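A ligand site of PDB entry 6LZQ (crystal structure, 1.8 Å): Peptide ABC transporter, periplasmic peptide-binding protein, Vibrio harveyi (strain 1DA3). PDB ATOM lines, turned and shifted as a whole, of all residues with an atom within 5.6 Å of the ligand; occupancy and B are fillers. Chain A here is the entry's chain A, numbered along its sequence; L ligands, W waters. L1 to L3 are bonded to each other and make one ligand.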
ATOM      1  N   HIS A   9      15.069 -10.573  18.015  1.00  0.00           N
ATOM      2  CA  HIS A   9      15.228  -9.470  18.973  1.00  0.00           C
ATOM      3  C   HIS A   9      16.181  -9.866  20.103  1.00  0.00           C
ATOM      4  O   HIS A   9      15.736 -10.247  21.180  1.00  0.00           O
ATOM      5  CB  HIS A   9      13.869  -9.046  19.554  1.00  0.00           C
ATOM      6  CG  HIS A   9      13.954  -7.869  20.480  1.00  0.00           C
ATOM      7  ND1 HIS A   9      14.850  -6.843  20.295  1.00  0.00           N
ATOM      8  CD2 HIS A   9      13.243  -7.564  21.593  1.00  0.00           C
ATOM      9  CE1 HIS A   9      14.699  -5.952  21.262  1.00  0.00           C
ATOM     10  NE2 HIS A   9      13.730  -6.367  22.065  1.00  0.00           N
ATOM     11  N   PRO A  10      17.491  -9.771  19.862  1.00  0.00           N
ATOM     12  CA  PRO A  10      18.436 -10.216  20.893  1.00  0.00           C
ATOM     13  C   PRO A  10      18.737  -9.194  21.997  1.00  0.00           C
ATOM     14  O   PRO A  10      19.200  -9.585  23.076  1.00  0.00           O
ATOM     15  CB  PRO A  10      19.716 -10.520  20.098  1.00  0.00           C
ATOM     16  CG  PRO A  10      19.631  -9.642  18.872  1.00  0.00           C
ATOM     17  CD  PRO A  10      18.150  -9.518  18.565  1.00  0.00           C
ATOM     18  N   LYS A  11      18.456  -7.927  21.767  1.00  0.00           N
ATOM     19  CA  LYS A  11      18.917  -6.881  22.700  1.00  0.00           C
ATOM     20  C   LYS A  11      18.183  -5.594  22.453  1.00  0.00           C
ATOM     21  O   LYS A  11      18.005  -5.182  21.309  1.00  0.00           O
ATOM     22  CB  LYS A  11      20.439  -6.680  22.552  1.00  0.00           C
ATOM     23  CG  LYS A  11      21.043  -5.491  23.311  1.00  0.00           C
ATOM     24  CD  LYS A  11      21.137  -5.745  24.806  1.00  0.00           C
ATOM     25  CE  LYS A  11      21.854  -4.571  25.515  1.00  0.00           C
ATOM     26  NZ  LYS A  11      21.892  -4.761  27.001  1.00  0.00           N
ATOM     27  N   GLU A  12      17.753  -4.920  23.521  1.00  0.00           N
ATOM     28  CA  GLU A  12      17.106  -3.641  23.309  1.00  0.00           C
ATOM     29  C   GLU A  12      18.145  -2.551  23.001  1.00  0.00           C
ATOM     30  O   GLU A  12      19.254  -2.554  23.546  1.00  0.00           O
ATOM     31  CB  GLU A  12      16.206  -3.259  24.505  1.00  0.00           C
ATOM     32  CG  GLU A  12      16.752  -3.485  25.895  1.00  0.00           C
ATOM     33  CD  GLU A  12      16.701  -4.940  26.380  1.00  0.00           C
ATOM     34  OE1 GLU A  12      17.742  -5.583  26.261  1.00  0.00           O
ATOM     35  OE2 GLU A  12      15.664  -5.429  26.895  1.00  0.00           O
ATOM     36  N   GLY A  25      31.673  -5.733  23.801  1.00  0.00           N
ATOM     37  CA  GLY A  25      30.346  -6.082  24.255  1.00  0.00           C
ATOM     38  C   GLY A  25      29.504  -4.932  24.752  1.00  0.00           C
ATOM     39  O   GLY A  25      28.265  -5.020  24.765  1.00  0.00           O
ATOM     40  N   ALA A  26      30.142  -3.842  25.157  1.00  0.00           N
ATOM     41  CA  ALA A  26      29.405  -2.681  25.647  1.00  0.00           C
ATOM     42  C   ALA A  26      28.738  -1.880  24.531  1.00  0.00           C
ATOM     43  O   ALA A  26      27.815  -1.107  24.785  1.00  0.00           O
ATOM     44  CB  ALA A  26      30.317  -1.788  26.470  1.00  0.00           C
ATOM     45  N   ASN A  28      28.667  -3.170  20.803  1.00  0.00           N
ATOM     46  CA  ASN A  28      28.376  -3.826  19.529  1.00  0.00           C
ATOM     47  C   ASN A  28      26.906  -4.218  19.382  1.00  0.00           C
ATOM     48  O   ASN A  28      26.110  -4.095  20.321  1.00  0.00           O
ATOM     49  CB  ASN A  28      29.262  -5.063  19.318  1.00  0.00           C
ATOM     50  CG  ASN A  28      29.063  -6.139  20.364  1.00  0.00           C
ATOM     51  OD1 ASN A  28      28.065  -6.174  21.083  1.00  0.00           O
ATOM     52  ND2 ASN A  28      30.030  -7.042  20.447  1.00  0.00           N
ATOM     53  N   HIS A  30      24.110  -7.220  18.795  1.00  0.00           N
ATOM     54  CA  HIS A  30      24.082  -8.533  19.419  1.00  0.00           C
ATOM     55  C   HIS A  30      23.735  -9.654  18.473  1.00  0.00           C
ATOM     56  O   HIS A  30      23.186 -10.673  18.869  1.00  0.00           O
ATOM     57  CB  HIS A  30      23.123  -8.519  20.592  1.00  0.00           C
ATOM     58  CG  HIS A  30      23.663  -7.784  21.770  1.00  0.00           C
ATOM     59  ND1 HIS A  30      23.422  -8.178  23.065  1.00  0.00           N
ATOM     60  CD2 HIS A  30      24.423  -6.659  21.846  1.00  0.00           C
ATOM     61  CE1 HIS A  30      24.007  -7.341  23.893  1.00  0.00           C
ATOM     62  NE2 HIS A  30      24.626  -6.407  23.177  1.00  0.00           N
ATOM     63  N   THR A  33      28.457 -12.134  17.613  1.00  0.00           N
ATOM     64  CA  THR A  33      28.883 -13.442  18.065  1.00  0.00           C
ATOM     65  C   THR A  33      27.899 -14.490  17.553  1.00  0.00           C
ATOM     66  O   THR A  33      26.717 -14.195  17.378  1.00  0.00           O
ATOM     67  CB  THR A  33      29.022 -13.501  19.593  1.00  0.00           C
ATOM     68  OG1 THR A  33      27.770 -13.161  20.204  1.00  0.00           O
ATOM     69  CG2 THR A  33      30.084 -12.492  20.076  1.00  0.00           C
ATOM     70  N   GLN A 104      36.443 -10.530  27.910  1.00  0.00           N
ATOM     71  CA  GLN A 104      35.162 -10.336  28.580  1.00  0.00           C
ATOM     72  C   GLN A 104      34.806 -11.487  29.506  1.00  0.00           C
ATOM     73  O   GLN A 104      33.794 -11.421  30.189  1.00  0.00           O
ATOM     74  CB  GLN A 104      34.062 -10.125  27.531  1.00  0.00           C
ATOM     75  CG  GLN A 104      34.354  -9.000  26.567  1.00  0.00           C
ATOM     76  CD  GLN A 104      33.188  -8.707  25.653  1.00  0.00           C
ATOM     77  OE1 GLN A 104      32.294  -7.926  25.999  1.00  0.00           O
ATOM     78  NE2 GLN A 104      33.177  -9.327  24.481  1.00  0.00           N
ATOM     79  N   ASN A 206      10.380  -3.105  27.131  1.00  0.00           N
ATOM     80  CA  ASN A 206       9.386  -4.176  27.105  1.00  0.00           C
ATOM     81  C   ASN A 206       8.018  -3.698  26.619  1.00  0.00           C
ATOM     82  O   ASN A 206       7.256  -4.476  26.062  1.00  0.00           O
ATOM     83  CB  ASN A 206       9.260  -4.805  28.489  1.00  0.00           C
ATOM     84  CG  ASN A 206      10.395  -5.765  28.826  1.00  0.00           C
ATOM     85  OD1 ASN A 206      11.260  -6.033  27.982  1.00  0.00           O
ATOM     86  ND2 ASN A 206      10.405  -6.285  30.058  1.00  0.00           N
ATOM     87  N   SER A 222      13.007 -13.350  23.057  1.00  0.00           N
ATOM     88  CA  SER A 222      13.248 -13.875  24.390  1.00  0.00           C
ATOM     89  C   SER A 222      12.981 -12.809  25.473  1.00  0.00           C
ATOM     90  O   SER A 222      13.647 -12.797  26.501  1.00  0.00           O
ATOM     91  CB  SER A 222      14.697 -14.364  24.505  1.00  0.00           C
ATOM     92  OG  SER A 222      14.916 -15.502  23.682  1.00  0.00           O
ATOM     93  N   SER A 223      11.997 -11.950  25.226  1.00  0.00           N
ATOM     94  CA  SER A 223      11.712 -10.842  26.146  1.00  0.00           C
ATOM     95  C   SER A 223      10.699 -11.215  27.200  1.00  0.00           C
ATOM     96  O   SER A 223       9.956 -12.188  27.064  1.00  0.00           O
ATOM     97  CB  SER A 223      11.159  -9.626  25.373  1.00  0.00           C
ATOM     98  OG  SER A 223      12.142  -9.081  24.506  1.00  0.00           O
ATOM     99  N   PHE A 224      10.659 -10.428  28.267  1.00  0.00           N
ATOM    100  CA  PHE A 224       9.603 -10.595  29.230  1.00  0.00           C
ATOM    101  C   PHE A 224       8.277 -10.130  28.613  1.00  0.00           C
ATOM    102  O   PHE A 224       8.208  -9.055  28.001  1.00  0.00           O
ATOM    103  CB  PHE A 224       9.869  -9.817  30.523  1.00  0.00           C
ATOM    104  CG  PHE A 224       8.695  -9.802  31.444  1.00  0.00           C
ATOM    105  CD1 PHE A 224       8.360 -10.931  32.193  1.00  0.00           C
ATOM    106  CD2 PHE A 224       7.885  -8.672  31.536  1.00  0.00           C
ATOM    107  CE1 PHE A 224       7.261 -10.933  33.029  1.00  0.00           C
ATOM    108  CE2 PHE A 224       6.786  -8.674  32.372  1.00  0.00           C
ATOM    109  CZ  PHE A 224       6.476  -9.800  33.121  1.00  0.00           C
ATOM    110  N   GLN A 249      18.312 -14.985  40.419  1.00  0.00           N
ATOM    111  CA  GLN A 249      18.211 -13.537  40.446  1.00  0.00           C
ATOM    112  C   GLN A 249      18.319 -13.079  41.890  1.00  0.00           C
ATOM    113  O   GLN A 249      17.810 -13.756  42.783  1.00  0.00           O
ATOM    114  CB  GLN A 249      16.899 -13.055  39.833  1.00  0.00           C
ATOM    115  CG  GLN A 249      16.754 -13.512  38.371  1.00  0.00           C
ATOM    116  CD  GLN A 249      15.441 -13.088  37.753  1.00  0.00           C
ATOM    117  OE1 GLN A 249      14.730 -12.246  38.309  1.00  0.00           O
ATOM    118  NE2 GLN A 249      15.135 -13.640  36.582  1.00  0.00           N
ATOM    119  N   PHE A 289       6.361 -11.519  37.854  1.00  0.00           N
ATOM    120  CA  PHE A 289       6.674 -12.476  36.805  1.00  0.00           C
ATOM    121  C   PHE A 289       5.480 -13.319  36.381  1.00  0.00           C
ATOM    122  O   PHE A 289       5.626 -14.233  35.580  1.00  0.00           O
ATOM    123  CB  PHE A 289       7.813 -13.390  37.269  1.00  0.00           C
ATOM    124  CG  PHE A 289       9.113 -12.673  37.460  1.00  0.00           C
ATOM    125  CD1 PHE A 289       9.434 -12.113  38.688  1.00  0.00           C
ATOM    126  CD2 PHE A 289       9.989 -12.524  36.399  1.00  0.00           C
ATOM    127  CE1 PHE A 289      10.631 -11.423  38.870  1.00  0.00           C
ATOM    128  CE2 PHE A 289      11.190 -11.840  36.587  1.00  0.00           C
ATOM    129  CZ  PHE A 289      11.512 -11.279  37.816  1.00  0.00           C
ATOM    130  N   GLY A 364      13.503  -0.314  31.171  1.00  0.00           N
ATOM    131  CA  GLY A 364      12.786  -1.152  30.226  1.00  0.00           C
ATOM    132  C   GLY A 364      12.712  -2.630  30.557  1.00  0.00           C
ATOM    133  O   GLY A 364      11.940  -3.356  29.917  1.00  0.00           O
ATOM    134  N   TRP A 365      13.482  -3.093  31.548  1.00  0.00           N
ATOM    135  CA  TRP A 365      13.342  -4.491  31.996  1.00  0.00           C
ATOM    136  C   TRP A 365      12.244  -4.530  33.040  1.00  0.00           C
ATOM    137  O   TRP A 365      12.521  -4.623  34.242  1.00  0.00           O
ATOM    138  CB  TRP A 365      14.642  -5.057  32.574  1.00  0.00           C
ATOM    139  CG  TRP A 365      15.845  -5.112  31.658  1.00  0.00           C
ATOM    140  CD1 TRP A 365      16.065  -4.389  30.530  1.00  0.00           C
ATOM    141  CD2 TRP A 365      17.002  -5.939  31.838  1.00  0.00           C
ATOM    142  NE1 TRP A 365      17.279  -4.717  29.988  1.00  0.00           N
ATOM    143  CE2 TRP A 365      17.878  -5.668  30.779  1.00  0.00           C
ATOM    144  CE3 TRP A 365      17.381  -6.892  32.803  1.00  0.00           C
ATOM    145  CZ2 TRP A 365      19.099  -6.308  30.638  1.00  0.00           C
ATOM    146  CZ3 TRP A 365      18.593  -7.532  32.668  1.00  0.00           C
ATOM    147  CH2 TRP A 365      19.450  -7.237  31.582  1.00  0.00           C
ATOM    148  N   THR A 366      11.003  -4.464  32.586  1.00  0.00           N
ATOM    149  CA  THR A 366       9.901  -4.165  33.476  1.00  0.00           C
ATOM    150  C   THR A 366       9.636  -5.194  34.551  1.00  0.00           C
ATOM    151  O   THR A 366       9.202  -4.838  35.660  1.00  0.00           O
ATOM    152  CB  THR A 366       8.628  -3.941  32.669  1.00  0.00           C
ATOM    153  OG1 THR A 366       8.379  -5.087  31.843  1.00  0.00           O
ATOM    154  CG2 THR A 366       8.786  -2.704  31.794  1.00  0.00           C
ATOM    155  N   ASP A 367       9.886  -6.480  34.271  1.00  0.00           N
ATOM    156  CA  ASP A 367       9.738  -7.495  35.304  1.00  0.00           C
ATOM    157  C   ASP A 367      10.708  -7.209  36.473  1.00  0.00           C
ATOM    158  O   ASP A 367      10.326  -7.363  37.643  1.00  0.00           O
ATOM    159  CB  ASP A 367       9.960  -8.919  34.756  1.00  0.00           C
ATOM    160  CG  ASP A 367      11.230  -9.059  33.899  1.00  0.00           C
ATOM    161  OD1 ASP A 367      11.781  -8.052  33.417  1.00  0.00           O
ATOM    162  OD2 ASP A 367      11.672 -10.216  33.685  1.00  0.00           O
ATOM    163  N   PHE A 368      11.929  -6.781  36.165  1.00  0.00           N
ATOM    164  CA  PHE A 368      12.880  -6.431  37.239  1.00  0.00           C
ATOM    165  C   PHE A 368      12.485  -5.116  37.921  1.00  0.00           C
ATOM    166  O   PHE A 368      12.633  -4.970  39.138  1.00  0.00           O
ATOM    167  CB  PHE A 368      14.321  -6.311  36.698  1.00  0.00           C
ATOM    168  CG  PHE A 368      14.955  -7.619  36.320  1.00  0.00           C
ATOM    169  CD1 PHE A 368      14.203  -8.774  36.167  1.00  0.00           C
ATOM    170  CD2 PHE A 368      16.334  -7.698  36.119  1.00  0.00           C
ATOM    171  CE1 PHE A 368      14.811  -9.996  35.805  1.00  0.00           C
ATOM    172  CE2 PHE A 368      16.944  -8.898  35.761  1.00  0.00           C
ATOM    173  CZ  PHE A 368      16.175 -10.056  35.602  1.00  0.00           C
ATOM    174  N   ASN A 411      19.963 -10.591  37.289  1.00  0.00           N
ATOM    175  CA  ASN A 411      20.064 -12.018  37.038  1.00  0.00           C
ATOM    176  C   ASN A 411      21.499 -12.400  36.773  1.00  0.00           C
ATOM    177  O   ASN A 411      22.389 -11.543  36.732  1.00  0.00           O
ATOM    178  CB  ASN A 411      19.159 -12.454  35.871  1.00  0.00           C
ATOM    179  CG  ASN A 411      19.363 -11.629  34.602  1.00  0.00           C
ATOM    180  OD1 ASN A 411      19.989 -10.571  34.609  1.00  0.00           O
ATOM    181  ND2 ASN A 411      18.791 -12.106  33.506  1.00  0.00           N
ATOM    182  N   TYR A 412      21.732 -13.709  36.606  1.00  0.00           N
ATOM    183  CA  TYR A 412      23.070 -14.251  36.407  1.00  0.00           C
ATOM    184  C   TYR A 412      23.082 -15.282  35.312  1.00  0.00           C
ATOM    185  O   TYR A 412      22.037 -15.889  35.034  1.00  0.00           O
ATOM    186  CB  TYR A 412      23.568 -14.923  37.668  1.00  0.00           C
ATOM    187  CG  TYR A 412      23.768 -14.030  38.852  1.00  0.00           C
ATOM    188  CD1 TYR A 412      24.975 -13.401  39.048  1.00  0.00           C
ATOM    189  CD2 TYR A 412      22.762 -13.858  39.789  1.00  0.00           C
ATOM    190  CE1 TYR A 412      25.187 -12.597  40.144  1.00  0.00           C
ATOM    191  CE2 TYR A 412      22.964 -13.038  40.907  1.00  0.00           C
ATOM    192  CZ  TYR A 412      24.189 -12.425  41.075  1.00  0.00           C
ATOM    193  OH  TYR A 412      24.431 -11.627  42.161  1.00  0.00           O
ATOM    194  N   PHE A 413      24.260 -15.536  34.754  1.00  0.00           N
ATOM    195  CA  PHE A 413      24.469 -16.701  33.900  1.00  0.00           C
ATOM    196  C   PHE A 413      24.076 -17.941  34.668  1.00  0.00           C
ATOM    197  O   PHE A 413      24.198 -18.012  35.895  1.00  0.00           O
ATOM    198  CB  PHE A 413      25.933 -16.831  33.456  1.00  0.00           C
ATOM    199  CG  PHE A 413      26.466 -15.633  32.746  1.00  0.00           C
ATOM    200  CD1 PHE A 413      25.688 -14.929  31.851  1.00  0.00           C
ATOM    201  CD2 PHE A 413      27.770 -15.220  32.970  1.00  0.00           C
ATOM    202  CE1 PHE A 413      26.193 -13.821  31.188  1.00  0.00           C
ATOM    203  CE2 PHE A 413      28.294 -14.121  32.331  1.00  0.00           C
ATOM    204  CZ  PHE A 413      27.507 -13.420  31.425  1.00  0.00           C
ATOM    205  N   ARG A 438      28.934  -7.022  35.102  1.00  0.00           N
ATOM    206  CA  ARG A 438      28.521  -6.536  36.415  1.00  0.00           C
ATOM    207  C   ARG A 438      28.490  -7.569  37.544  1.00  0.00           C
ATOM    208  O   ARG A 438      28.400  -7.195  38.724  1.00  0.00           O
ATOM    209  CB  ARG A 438      27.118  -5.940  36.316  1.00  0.00           C
ATOM    210  CG  ARG A 438      26.055  -6.999  36.003  1.00  0.00           C
ATOM    211  CD  ARG A 438      24.729  -6.336  35.633  1.00  0.00           C
ATOM    212  NE  ARG A 438      23.622  -7.288  35.399  1.00  0.00           N
ATOM    213  CZ  ARG A 438      23.433  -7.924  34.251  1.00  0.00           C
ATOM    214  NH1 ARG A 438      24.247  -7.734  33.226  1.00  0.00           N
ATOM    215  NH2 ARG A 438      22.404  -8.756  34.113  1.00  0.00           N
ATOM    216  N   PHE A 439      28.504  -8.839  37.191  1.00  0.00           N
ATOM    217  CA  PHE A 439      27.958  -9.866  38.076  1.00  0.00           C
ATOM    218  C   PHE A 439      28.680 -10.016  39.406  1.00  0.00           C
ATOM    219  O   PHE A 439      28.042 -10.283  40.419  1.00  0.00           O
ATOM    220  CB  PHE A 439      27.923 -11.201  37.323  1.00  0.00           C
ATOM    221  CG  PHE A 439      27.073 -11.150  36.105  1.00  0.00           C
ATOM    222  CD1 PHE A 439      25.706 -10.954  36.204  1.00  0.00           C
ATOM    223  CD2 PHE A 439      27.636 -11.233  34.840  1.00  0.00           C
ATOM    224  CE1 PHE A 439      24.900 -10.893  35.083  1.00  0.00           C
ATOM    225  CE2 PHE A 439      26.841 -11.163  33.718  1.00  0.00           C
ATOM    226  CZ  PHE A 439      25.481 -10.985  33.842  1.00  0.00           C
ATOM    227  N   MET A 491      13.155 -16.967  28.918  1.00  0.00           N
ATOM    228  CA  MET A 491      11.964 -16.543  28.196  1.00  0.00           C
ATOM    229  C   MET A 491      12.191 -16.719  26.713  1.00  0.00           C
ATOM    230  O   MET A 491      13.255 -16.378  26.199  1.00  0.00           O
ATOM    231  CB  MET A 491      11.597 -15.094  28.506  1.00  0.00           C
ATOM    232  CG  MET A 491      11.457 -14.807  29.993  1.00  0.00           C
ATOM    233  SD  MET A 491      12.995 -14.133  30.657  1.00  0.00           S
ATOM    234  CE  MET A 491      12.952 -12.502  29.939  1.00  0.00           C
ATOM    235  N   TRP A 515      19.150 -14.267  22.681  1.00  0.00           N
ATOM    236  CA  TRP A 515      20.162 -13.360  23.246  1.00  0.00           C
ATOM    237  C   TRP A 515      21.584 -13.678  22.774  1.00  0.00           C
ATOM    238  O   TRP A 515      21.924 -14.834  22.589  1.00  0.00           O
ATOM    239  CB  TRP A 515      20.171 -13.432  24.781  1.00  0.00           C
ATOM    240  CG  TRP A 515      18.871 -13.177  25.442  1.00  0.00           C
ATOM    241  CD1 TRP A 515      17.927 -12.240  25.099  1.00  0.00           C
ATOM    242  CD2 TRP A 515      18.341 -13.883  26.566  1.00  0.00           C
ATOM    243  NE1 TRP A 515      16.853 -12.323  25.951  1.00  0.00           N
ATOM    244  CE2 TRP A 515      17.089 -13.326  26.869  1.00  0.00           C
ATOM    245  CE3 TRP A 515      18.816 -14.942  27.353  1.00  0.00           C
ATOM    246  CZ2 TRP A 515      16.303 -13.783  27.912  1.00  0.00           C
ATOM    247  CZ3 TRP A 515      18.038 -15.397  28.408  1.00  0.00           C
ATOM    248  CH2 TRP A 515      16.785 -14.830  28.674  1.00  0.00           C
ATOM    249  N   ALA A 516      22.415 -12.655  22.619  1.00  0.00           N
ATOM    250  CA  ALA A 516      23.844 -12.937  22.520  1.00  0.00           C
ATOM    251  C   ALA A 516      24.267 -13.596  23.832  1.00  0.00           C
ATOM    252  O   ALA A 516      23.616 -13.396  24.855  1.00  0.00           O
ATOM    253  CB  ALA A 516      24.646 -11.658  22.262  1.00  0.00           C
ATOM    254  N   GLY A 517      25.322 -14.405  23.799  1.00  0.00           N
ATOM    255  CA  GLY A 517      25.730 -15.153  24.982  1.00  0.00           C
ATOM    256  C   GLY A 517      25.016 -16.495  25.121  1.00  0.00           C
ATOM    257  O   GLY A 517      25.193 -17.216  26.101  1.00  0.00           O
ATOM    258  N   ILE A 518      24.189 -16.813  24.137  1.00  0.00           N
ATOM    259  CA  ILE A 518      23.562 -18.132  24.053  1.00  0.00           C
ATOM    260  C   ILE A 518      24.010 -18.751  22.733  1.00  0.00           C
ATOM    261  O   ILE A 518      23.341 -18.590  21.706  1.00  0.00           O
ATOM    262  CB  ILE A 518      22.025 -18.043  24.134  1.00  0.00           C
ATOM    263  CG1 ILE A 518      21.620 -17.284  25.395  1.00  0.00           C
ATOM    264  CG2 ILE A 518      21.394 -19.437  24.077  1.00  0.00           C
ATOM    265  CD1 ILE A 518      21.990 -17.980  26.682  1.00  0.00           C
HETATM  266  C1  LIG L   1      26.057 -11.704  27.076  1.00  0.00           C
HETATM  267  C2  LIG L   1      25.262 -10.605  26.374  1.00  0.00           C
HETATM  268  C3  LIG L   1      24.087 -10.158  27.251  1.00  0.00           C
HETATM  269  C4  LIG L   1      23.256 -11.348  27.713  1.00  0.00           C
HETATM  270  C5  LIG L   1      24.142 -12.429  28.320  1.00  0.00           C
HETATM  271  C6  LIG L   1      23.393 -13.700  28.653  1.00  0.00           C
HETATM  272  C7  LIG L   1      26.854  -9.408  24.945  1.00  0.00           C
HETATM  273  C8  LIG L   1      27.629  -8.145  24.752  1.00  0.00           C
HETATM  274  O1  LIG L   1      25.189 -12.788  27.402  1.00  0.00           O
HETATM  275  O2  LIG L   1      23.272  -9.227  26.536  1.00  0.00           O
HETATM  276  O3  LIG L   1      22.381 -10.864  28.738  1.00  0.00           O
HETATM  277  O4  LIG L   1      22.777 -14.268  27.494  1.00  0.00           O
HETATM  278  O5  LIG L   1      26.907 -10.337  24.151  1.00  0.00           O
HETATM  279  N1  LIG L   1      26.107  -9.466  26.053  1.00  0.00           N
HETATM  280  O6  LIG L   1      26.627 -11.205  28.238  1.00  0.00           O
HETATM  281  C1  LG2 L   2      21.018 -10.957  28.490  1.00  0.00           C
HETATM  282  C2  LG2 L   2      20.314 -10.937  29.832  1.00  0.00           C
HETATM  283  C3  LG2 L   2      18.811 -11.098  29.609  1.00  0.00           C
HETATM  284  C4  LG2 L   2      18.390  -9.934  28.710  1.00  0.00           C
HETATM  285  C5  LG2 L   2      19.202  -9.893  27.418  1.00  0.00           C
HETATM  286  C6  LG2 L   2      18.894  -8.671  26.594  1.00  0.00           C
HETATM  287  C7  LG2 L   2      21.697 -11.706  31.701  1.00  0.00           C
HETATM  288  C8  LG2 L   2      22.111 -12.877  32.554  1.00  0.00           C
HETATM  289  N1  LG2 L   2      20.808 -11.971  30.733  1.00  0.00           N
HETATM  290  O1  LG2 L   2      18.157 -11.012  30.868  1.00  0.00           O
HETATM  291  O2  LG2 L   2      16.996 -10.091  28.382  1.00  0.00           O
HETATM  292  O3  LG2 L   2      20.603  -9.847  27.720  1.00  0.00           O
HETATM  293  O4  LG2 L   2      18.937  -7.487  27.390  1.00  0.00           O
HETATM  294  O5  LG2 L   2      22.141 -10.580  31.884  1.00  0.00           O
HETATM  295  C1  LG3 L   3      16.109  -9.202  29.000  1.00  0.00           C
HETATM  296  C2  LG3 L   3      14.893  -9.056  28.098  1.00  0.00           C
HETATM  297  C3  LG3 L   3      13.819  -8.224  28.815  1.00  0.00           C
HETATM  298  C4  LG3 L   3      13.587  -8.663  30.262  1.00  0.00           C
HETATM  299  C5  LG3 L   3      14.923  -8.791  30.987  1.00  0.00           C
HETATM  300  C6  LG3 L   3      14.799  -9.307  32.409  1.00  0.00           C
HETATM  301  C7  LG3 L   3      15.256  -9.029  25.635  1.00  0.00           C
HETATM  302  C8  LG3 L   3      15.544  -8.142  24.451  1.00  0.00           C
HETATM  303  N1  LG3 L   3      15.252  -8.421  26.837  1.00  0.00           N
HETATM  304  O1  LG3 L   3      12.604  -8.314  28.084  1.00  0.00           O
HETATM  305  O2  LG3 L   3      12.820  -7.669  30.930  1.00  0.00           O
HETATM  306  O3  LG3 L   3      15.753  -9.720  30.269  1.00  0.00           O
HETATM  307  O4  LG3 L   3      14.046 -10.522  32.462  1.00  0.00           O
HETATM  308  O5  LG3 L   3      15.052 -10.239  25.493  1.00  0.00           O
HETATM  309  O   HOH W   1      13.817 -10.775  23.114  1.00  0.00           O
HETATM  310  O   HOH W   2      21.846 -10.016  23.967  1.00  0.00           O
HETATM  311  O   HOH W   3      29.944 -11.529  27.362  1.00  0.00           O
HETATM  312  O   HOH W   4      21.935  -7.374  28.097  1.00  0.00           O
HETATM  313  O   HOH W   5      27.306  -8.967  21.404  1.00  0.00           O
HETATM  314  O   HOH W   6      23.194  -8.456  30.371  1.00  0.00           O
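O4 of LG2 L2 is in hydrogen-bond range of OE1 of Glu 12 (2.5 Å).
The side-chain amide oxygen (OD1) of Asn 206 sits at hydrogen-bond distance from an oxygen (O1) of LG3 L3 (2.6 Å).
An oxygen (O4) of LG3 L3 is in hydrogen-bond range of the side-chain carboxylate (OD2) of Asp 367, at 2.7 Å.
The indole nitrogen (NE1) of Trp 515 sits at hydrogen-bond distance from an oxygen (O5) of LG3 L3, at 2.8 Å.
An oxygen (O1) of LG3 L3 is in hydrogen-bond range of the backbone NH (N) of Phe 224, at 2.9 Å.
The guanidinium group (NH2) of Arg 438 is in hydrogen-bond range of an oxygen (O5) of LG2 L2 (2.9 Å).
The backbone carbonyl oxygen of Ala 516 sits at hydrogen-bond distance from an oxygen (O4) of LIG L1, at 2.9 Å.
The side-chain amide nitrogen (ND2) of Asn 411 is in hydrogen-bond range of an oxygen (O1) of LG2 L2, at 2.9 Å.
O5 of LG3 L3 lies within hydrogen-bond range of OG of Ser 223 (3.3 Å).
The side-chain amide nitrogen of Asn 206 sits at hydrogen-bond distance from the side-chain hydroxyl of Thr 366.
The backbone NH of Asn 206 sits close to the backbone carbonyl oxygen of Gly 364, 3.2 Å away.
The indole nitrogen (NE1) of Trp 515 lies close to the backbone carbonyl oxygen (O) of Ser 222.
OD1 of Asn 411 is in hydrogen-bond range of NH2 of Arg 438 (3.1 Å).
The side-chain hydroxyl (OG) of Ser 222 lies close to the backbone carbonyl oxygen (O) of Met 491 (3.1 Å).
The backbone NH of Gly 25 lies within hydrogen-bond range of the side-chain amide oxygen of Gln 104 (3.2 Å).
The backbone carbonyl oxygen (O) of Ser 222 sits close to an oxygen (O5) of LG3 L3, 3.1 Å away.
Merely in contact with the ligand: His 9 (3.5 Å), Pro 10 (3.6 Å), Lys 11 (3.8 Å), Gly 25 (3.2 Å), His 30 (3.3 Å), Trp 365 (3.4 Å), Phe 368 (3.5 Å), Tyr 412 (3.8 Å), Phe 413 (3.8 Å), Phe 439 (3.9 Å), Met 491 (3.4 Å), Gly 517 (3.4 Å) and Ile 518 (3.9 Å).
Hydrophobic or aromatic side chains that line the ligand: His 9, His 30, Phe 224, Trp 365, Phe 368, Phe 413, Phe 439, Met 491, Trp 515, Ala 516 and Ile 518.
Within 4 Å of the ligand: His 9, Pro 10, Lys 11, Glu 12, Gly 25, His 30, Asn 206, Ser 222, Ser 223, Phe 224, Trp 365, Asp 367, Phe 368, Asn 411, Tyr 412, Phe 413, Arg 438, Phe 439, Met 491, Trp 515, Ala 516, Gly 517 and Ile 518.
Water W1 lies within hydrogen-bond range of N of Ser 222, O5 of LG3 L3, OG of Ser 223 and O of His 9.
Water W4 bridges O2 of LIG L1 and NZ of Lys 11.
Water W6 lies within hydrogen-bond range of O5 of LG2 L2 (2.8 Å) and NH1 of Arg 438 (3.1 Å).
Water W2 lies within hydrogen-bond range of a ring nitrogen (ND1) of His 30, the backbone carbonyl oxygen (O) of Pro 10, the backbone NH (N) of Ala 516 and an oxygen (O2) of LIG L1.
Water W5 lies within hydrogen-bond range of the side-chain amide oxygen (OD1) of Asn 28 (2.9 Å) and an oxygen (O5) of LIG L1 (3.1 Å).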
